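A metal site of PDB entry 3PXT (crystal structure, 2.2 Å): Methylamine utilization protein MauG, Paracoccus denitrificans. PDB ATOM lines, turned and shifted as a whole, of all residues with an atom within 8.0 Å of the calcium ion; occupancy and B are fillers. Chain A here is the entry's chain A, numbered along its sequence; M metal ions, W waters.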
ATOM      1  N   ARG A  39      -0.416  -2.447  -4.160  1.00  0.00           N
ATOM      2  CA  ARG A  39      -1.497  -3.437  -3.972  1.00  0.00           C
ATOM      3  C   ARG A  39      -2.027  -4.019  -5.288  1.00  0.00           C
ATOM      4  O   ARG A  39      -3.236  -4.195  -5.457  1.00  0.00           O
ATOM      5  CB  ARG A  39      -2.642  -2.857  -3.126  1.00  0.00           C
ATOM      6  CG  ARG A  39      -3.187  -3.834  -2.083  1.00  0.00           C
ATOM      7  CD  ARG A  39      -4.405  -3.302  -1.338  1.00  0.00           C
ATOM      8  NE  ARG A  39      -5.606  -3.594  -2.103  1.00  0.00           N
ATOM      9  CZ  ARG A  39      -6.577  -4.435  -1.730  1.00  0.00           C
ATOM     10  NH1 ARG A  39      -6.545  -5.058  -0.557  1.00  0.00           N
ATOM     11  NH2 ARG A  39      -7.597  -4.616  -2.539  1.00  0.00           N
ATOM     12  N   THR A  42      -4.736  -1.906  -7.211  1.00  0.00           N
ATOM     13  CA  THR A  42      -6.070  -1.769  -6.610  1.00  0.00           C
ATOM     14  C   THR A  42      -6.020  -0.800  -5.418  1.00  0.00           C
ATOM     15  O   THR A  42      -4.969  -0.247  -5.101  1.00  0.00           O
ATOM     16  CB  THR A  42      -6.642  -3.121  -6.138  1.00  0.00           C
ATOM     17  OG1 THR A  42      -5.794  -3.674  -5.125  1.00  0.00           O
ATOM     18  CG2 THR A  42      -6.793  -4.108  -7.301  1.00  0.00           C
ATOM     19  N   ASP A  43      -7.156  -0.613  -4.753  1.00  0.00           N
ATOM     20  CA  ASP A  43      -7.320   0.440  -3.754  1.00  0.00           C
ATOM     21  C   ASP A  43      -7.261  -0.094  -2.319  1.00  0.00           C
ATOM     22  O   ASP A  43      -8.173  -0.812  -1.875  1.00  0.00           O
ATOM     23  CB  ASP A  43      -8.614   1.202  -4.002  1.00  0.00           C
ATOM     24  CG  ASP A  43      -8.679   2.543  -3.257  1.00  0.00           C
ATOM     25  OD1 ASP A  43      -9.663   3.281  -3.478  1.00  0.00           O
ATOM     26  OD2 ASP A  43      -7.765   2.861  -2.462  1.00  0.00           O
ATOM     27  N   LEU A  51     -13.446  -1.760   1.763  1.00  0.00           N
ATOM     28  CA  LEU A  51     -12.615  -1.690   0.558  1.00  0.00           C
ATOM     29  C   LEU A  51     -13.389  -2.082  -0.703  1.00  0.00           C
ATOM     30  O   LEU A  51     -12.799  -2.249  -1.776  1.00  0.00           O
ATOM     31  CB  LEU A  51     -11.370  -2.567   0.713  1.00  0.00           C
ATOM     32  CG  LEU A  51     -10.072  -1.923   1.209  1.00  0.00           C
ATOM     33  CD1 LEU A  51     -10.144  -1.523   2.680  1.00  0.00           C
ATOM     34  CD2 LEU A  51      -8.898  -2.856   0.973  1.00  0.00           C
ATOM     35  N   ALA A  52     -14.715  -2.209  -0.556  1.00  0.00           N
ATOM     36  CA  ALA A  52     -15.610  -2.594  -1.660  1.00  0.00           C
ATOM     37  C   ALA A  52     -15.646  -1.592  -2.805  1.00  0.00           C
ATOM     38  O   ALA A  52     -15.728  -1.988  -3.974  1.00  0.00           O
ATOM     39  CB  ALA A  52     -17.027  -2.845  -1.132  1.00  0.00           C
ATOM     40  N   ASN A  66     -16.300  -2.152  -7.492  1.00  0.00           N
ATOM     41  CA  ASN A  66     -14.969  -2.370  -6.948  1.00  0.00           C
ATOM     42  C   ASN A  66     -13.883  -2.044  -7.973  1.00  0.00           C
ATOM     43  O   ASN A  66     -14.021  -2.362  -9.161  1.00  0.00           O
ATOM     44  CB  ASN A  66     -14.853  -3.833  -6.507  1.00  0.00           C
ATOM     45  CG  ASN A  66     -13.514  -4.152  -5.875  1.00  0.00           C
ATOM     46  OD1 ASN A  66     -12.711  -4.915  -6.425  1.00  0.00           O
ATOM     47  ND2 ASN A  66     -13.262  -3.556  -4.703  1.00  0.00           N
ATOM     48  N   THR A  67     -12.809  -1.400  -7.499  1.00  0.00           N
ATOM     49  CA  THR A  67     -11.661  -1.087  -8.351  1.00  0.00           C
ATOM     50  C   THR A  67     -10.867  -2.351  -8.736  1.00  0.00           C
ATOM     51  O   THR A  67     -10.287  -3.008  -7.869  1.00  0.00           O
ATOM     52  CB  THR A  67     -10.713  -0.069  -7.674  1.00  0.00           C
ATOM     53  OG1 THR A  67     -11.434   1.129  -7.376  1.00  0.00           O
ATOM     54  CG2 THR A  67      -9.539   0.282  -8.585  1.00  0.00           C
ATOM     55  N   PRO A  68     -10.833  -2.680 -10.042  1.00  0.00           N
ATOM     56  CA  PRO A  68     -10.105  -3.866 -10.497  1.00  0.00           C
ATOM     57  C   PRO A  68      -8.614  -3.576 -10.724  1.00  0.00           C
ATOM     58  O   PRO A  68      -8.234  -2.423 -10.939  1.00  0.00           O
ATOM     59  CB  PRO A  68     -10.784  -4.182 -11.835  1.00  0.00           C
ATOM     60  CG  PRO A  68     -11.185  -2.828 -12.366  1.00  0.00           C
ATOM     61  CD  PRO A  68     -11.433  -1.933 -11.166  1.00  0.00           C
ATOM     62  N   THR A  69      -7.805  -4.627 -10.673  1.00  0.00           N
ATOM     63  CA  THR A  69      -6.384  -4.532 -11.032  1.00  0.00           C
ATOM     64  C   THR A  69      -6.178  -4.062 -12.461  1.00  0.00           C
ATOM     65  O   THR A  69      -6.995  -4.328 -13.350  1.00  0.00           O
ATOM     66  CB  THR A  69      -5.649  -5.890 -10.824  1.00  0.00           C
ATOM     67  OG1 THR A  69      -4.245  -5.712 -11.050  1.00  0.00           O
ATOM     68  CG2 THR A  69      -6.186  -6.985 -11.766  1.00  0.00           C
ATOM     69  N   TRP A  93     -16.026  -3.313 -15.718  1.00  0.00           N
ATOM     70  CA  TRP A  93     -16.791  -4.505 -15.361  1.00  0.00           C
ATOM     71  C   TRP A  93     -17.934  -4.766 -16.342  1.00  0.00           C
ATOM     72  O   TRP A  93     -18.300  -5.907 -16.573  1.00  0.00           O
ATOM     73  CB  TRP A  93     -17.362  -4.376 -13.931  1.00  0.00           C
ATOM     74  CG  TRP A  93     -16.368  -4.540 -12.816  1.00  0.00           C
ATOM     75  CD1 TRP A  93     -15.777  -3.546 -12.104  1.00  0.00           C
ATOM     76  CD2 TRP A  93     -15.868  -5.769 -12.274  1.00  0.00           C
ATOM     77  NE1 TRP A  93     -14.923  -4.072 -11.149  1.00  0.00           N
ATOM     78  CE2 TRP A  93     -14.971  -5.440 -11.228  1.00  0.00           C
ATOM     79  CE3 TRP A  93     -16.092  -7.127 -12.554  1.00  0.00           C
ATOM     80  CZ2 TRP A  93     -14.300  -6.406 -10.476  1.00  0.00           C
ATOM     81  CZ3 TRP A  93     -15.424  -8.103 -11.793  1.00  0.00           C
ATOM     82  CH2 TRP A  93     -14.543  -7.725 -10.772  1.00  0.00           C
ATOM     83  N   ASN A 271      -3.164 -12.393  -9.620  1.00  0.00           N
ATOM     84  CA  ASN A 271      -3.085 -11.555  -8.427  1.00  0.00           C
ATOM     85  C   ASN A 271      -4.342 -11.587  -7.549  1.00  0.00           C
ATOM     86  O   ASN A 271      -4.440 -10.822  -6.578  1.00  0.00           O
ATOM     87  CB  ASN A 271      -2.702 -10.120  -8.779  1.00  0.00           C
ATOM     88  CG  ASN A 271      -1.257 -10.007  -9.234  1.00  0.00           C
ATOM     89  OD1 ASN A 271      -0.373 -10.681  -8.708  1.00  0.00           O
ATOM     90  ND2 ASN A 271      -1.008  -9.124 -10.202  1.00  0.00           N
ATOM     91  N   VAL A 272      -5.271 -12.485  -7.848  1.00  0.00           N
ATOM     92  CA  VAL A 272      -6.549 -12.546  -7.132  1.00  0.00           C
ATOM     93  C   VAL A 272      -6.381 -12.638  -5.615  1.00  0.00           C
ATOM     94  O   VAL A 272      -7.184 -12.081  -4.855  1.00  0.00           O
ATOM     95  CB  VAL A 272      -7.514 -13.662  -7.694  1.00  0.00           C
ATOM     96  CG1 VAL A 272      -7.048 -15.069  -7.320  1.00  0.00           C
ATOM     97  CG2 VAL A 272      -8.945 -13.429  -7.235  1.00  0.00           C
ATOM     98  N   VAL A 274      -4.436 -11.151  -3.686  1.00  0.00           N
ATOM     99  CA  VAL A 274      -4.093  -9.877  -3.043  1.00  0.00           C
ATOM    100  C   VAL A 274      -4.961  -8.685  -3.466  1.00  0.00           C
ATOM    101  O   VAL A 274      -4.628  -7.529  -3.150  1.00  0.00           O
ATOM    102  CB  VAL A 274      -2.591  -9.538  -3.228  1.00  0.00           C
ATOM    103  CG1 VAL A 274      -1.718 -10.567  -2.528  1.00  0.00           C
ATOM    104  CG2 VAL A 274      -2.221  -9.423  -4.705  1.00  0.00           C
ATOM    105  N   THR A 275      -6.050  -8.949  -4.185  1.00  0.00           N
ATOM    106  CA  THR A 275      -6.913  -7.875  -4.684  1.00  0.00           C
ATOM    107  C   THR A 275      -8.335  -7.952  -4.140  1.00  0.00           C
ATOM    108  O   THR A 275      -9.292  -7.483  -4.789  1.00  0.00           O
ATOM    109  CB  THR A 275      -6.982  -7.824  -6.235  1.00  0.00           C
ATOM    110  OG1 THR A 275      -7.688  -8.984  -6.710  1.00  0.00           O
ATOM    111  CG2 THR A 275      -5.586  -7.784  -6.846  1.00  0.00           C
ATOM    112  N   GLY A 276      -8.485  -8.547  -2.959  1.00  0.00           N
ATOM    113  CA  GLY A 276      -9.764  -8.533  -2.244  1.00  0.00           C
ATOM    114  C   GLY A 276     -10.155  -7.105  -1.909  1.00  0.00           C
ATOM    115  O   GLY A 276      -9.280  -6.243  -1.839  1.00  0.00           O
ATOM    116  N   PRO A 277     -11.462  -6.835  -1.702  1.00  0.00           N
ATOM    117  CA  PRO A 277     -12.587  -7.770  -1.743  1.00  0.00           C
ATOM    118  C   PRO A 277     -13.000  -8.140  -3.178  1.00  0.00           C
ATOM    119  O   PRO A 277     -12.450  -7.592  -4.136  1.00  0.00           O
ATOM    120  CB  PRO A 277     -13.703  -7.014  -1.016  1.00  0.00           C
ATOM    121  CG  PRO A 277     -13.394  -5.588  -1.258  1.00  0.00           C
ATOM    122  CD  PRO A 277     -11.908  -5.465  -1.380  1.00  0.00           C
ATOM    123  N   TYR A 278     -13.966  -9.042  -3.312  1.00  0.00           N
ATOM    124  CA  TYR A 278     -14.173  -9.721  -4.580  1.00  0.00           C
ATOM    125  C   TYR A 278     -15.501  -9.440  -5.278  1.00  0.00           C
ATOM    126  O   TYR A 278     -16.471  -9.033  -4.657  1.00  0.00           O
ATOM    127  CB  TYR A 278     -13.899 -11.229  -4.422  1.00  0.00           C
ATOM    128  CG  TYR A 278     -12.490 -11.446  -3.938  1.00  0.00           C
ATOM    129  CD1 TYR A 278     -12.217 -11.728  -2.602  1.00  0.00           C
ATOM    130  CD2 TYR A 278     -11.413 -11.290  -4.804  1.00  0.00           C
ATOM    131  CE1 TYR A 278     -10.920 -11.889  -2.140  1.00  0.00           C
ATOM    132  CE2 TYR A 278     -10.120 -11.457  -4.376  1.00  0.00           C
ATOM    133  CZ  TYR A 278      -9.875 -11.755  -3.048  1.00  0.00           C
ATOM    134  OH  TYR A 278      -8.565 -11.908  -2.630  1.00  0.00           O
ATOM    135  N   MET A 279     -15.496  -9.674  -6.594  1.00  0.00           N
ATOM    136  CA  MET A 279     -16.643  -9.439  -7.484  1.00  0.00           C
ATOM    137  C   MET A 279     -16.801  -7.957  -7.815  1.00  0.00           C
ATOM    138  O   MET A 279     -16.154  -7.091  -7.193  1.00  0.00           O
ATOM    139  CB  MET A 279     -17.939 -10.037  -6.907  1.00  0.00           C
ATOM    140  CG  MET A 279     -17.850 -11.514  -6.507  1.00  0.00           C
ATOM    141  SD  MET A 279     -17.281 -12.596  -7.830  1.00  0.00           S
ATOM    142  CE  MET A 279     -17.211 -14.157  -6.970  1.00  0.00           C
ATOM    143  N   HIS A 280     -17.666  -7.666  -8.788  1.00  0.00           N
ATOM    144  CA  HIS A 280     -17.861  -6.310  -9.313  1.00  0.00           C
ATOM    145  C   HIS A 280     -18.227  -5.267  -8.270  1.00  0.00           C
ATOM    146  O   HIS A 280     -17.975  -4.087  -8.469  1.00  0.00           O
ATOM    147  CB  HIS A 280     -18.893  -6.301 -10.460  1.00  0.00           C
ATOM    148  CG  HIS A 280     -20.281  -6.658 -10.031  1.00  0.00           C
ATOM    149  ND1 HIS A 280     -20.825  -7.911 -10.240  1.00  0.00           N
ATOM    150  CD2 HIS A 280     -21.246  -5.922  -9.429  1.00  0.00           C
ATOM    151  CE1 HIS A 280     -22.067  -7.933  -9.776  1.00  0.00           C
ATOM    152  NE2 HIS A 280     -22.341  -6.739  -9.276  1.00  0.00           N
ATOM    153  N   ASN A 281     -18.827  -5.710  -7.167  1.00  0.00           N
ATOM    154  CA  ASN A 281     -19.252  -4.812  -6.095  1.00  0.00           C
ATOM    155  C   ASN A 281     -18.531  -5.065  -4.760  1.00  0.00           C
ATOM    156  O   ASN A 281     -18.977  -4.593  -3.703  1.00  0.00           O
ATOM    157  CB  ASN A 281     -20.775  -4.905  -5.893  1.00  0.00           C
ATOM    158  CG  ASN A 281     -21.235  -6.302  -5.512  1.00  0.00           C
ATOM    159  OD1 ASN A 281     -20.427  -7.171  -5.201  1.00  0.00           O
ATOM    160  ND2 ASN A 281     -22.543  -6.510  -5.529  1.00  0.00           N
ATOM    161  N   GLY A 282     -17.430  -5.819  -4.815  1.00  0.00           N
ATOM    162  CA  GLY A 282     -16.598  -6.108  -3.643  1.00  0.00           C
ATOM    163  C   GLY A 282     -17.325  -6.681  -2.428  1.00  0.00           C
ATOM    164  O   GLY A 282     -16.925  -6.429  -1.298  1.00  0.00           O
ATOM    165  N   VAL A 283     -18.384  -7.445  -2.673  1.00  0.00           N
ATOM    166  CA  VAL A 283     -19.243  -7.960  -1.592  1.00  0.00           C
ATOM    167  C   VAL A 283     -18.510  -8.928  -0.653  1.00  0.00           C
ATOM    168  O   VAL A 283     -18.713  -8.901   0.569  1.00  0.00           O
ATOM    169  CB  VAL A 283     -20.580  -8.571  -2.144  1.00  0.00           C
ATOM    170  CG1 VAL A 283     -20.319  -9.715  -3.159  1.00  0.00           C
ATOM    171  CG2 VAL A 283     -21.505  -9.021  -1.020  1.00  0.00           C
ATOM    172  N   PHE A 284     -17.629  -9.757  -1.218  1.00  0.00           N
ATOM    173  CA  PHE A 284     -16.894 -10.747  -0.423  1.00  0.00           C
ATOM    174  C   PHE A 284     -15.482 -10.274  -0.116  1.00  0.00           C
ATOM    175  O   PHE A 284     -14.715  -9.981  -1.033  1.00  0.00           O
ATOM    176  CB  PHE A 284     -16.847 -12.104  -1.126  1.00  0.00           C
ATOM    177  CG  PHE A 284     -18.184 -12.583  -1.643  1.00  0.00           C
ATOM    178  CD1 PHE A 284     -19.325 -12.504  -0.847  1.00  0.00           C
ATOM    179  CD2 PHE A 284     -18.290 -13.124  -2.919  1.00  0.00           C
ATOM    180  CE1 PHE A 284     -20.556 -12.938  -1.334  1.00  0.00           C
ATOM    181  CE2 PHE A 284     -19.512 -13.565  -3.400  1.00  0.00           C
ATOM    182  CZ  PHE A 284     -20.649 -13.475  -2.613  1.00  0.00           C
HETATM  183 CA    CA M   1     -11.228  -6.714  -5.968  1.00  0.00          CA
HETATM  184  O   HOH W   1      -9.845  -5.570  -7.427  1.00  0.00           O
HETATM  185  O   HOH W   2     -10.193  -8.740  -7.133  1.00  0.00           O
HETATM  186  O   HOH W   3     -10.711  -4.813  -4.391  1.00  0.00           O
HETATM  187  O   HOH W   4     -12.931  -7.706  -7.450  1.00  0.00           O
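O of Asn 66 sits at hydrogen-bond distance from NE1 of Trp 93 (2.8 Å).
The backbone carbonyl oxygen of Leu 51 is in hydrogen-bond range of the side-chain amide nitrogen of Asn 66 (3.2 Å).
ND2 of Asn 66 lies within hydrogen-bond range of O of Ala 52, 3.0 Å away.
The backbone carbonyl oxygen (O) of His 280 is in hydrogen-bond range of the backbone NH (N) of Asn 66, at 2.7 Å.
Water W3 lies within hydrogen-bond range of ND2 of Asn 66 (2.9 Å) and O of Gly 276 (3.3 Å).
The calcium ion is bound by water W1 (2.3 Å), O of Pro 277 (2.4 Å), OD1 of Asn 66 (2.4 Å), O of Thr 275 (2.4 Å), water W4 (2.5 Å), water W3 (2.5 Å) and water W2 (2.6 Å).
Of the 23 residues printed, 3 come within 4 Å of the calcium ion.
Along chain A the residues within 4 Å of the calcium ion span positions 66 to 277.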
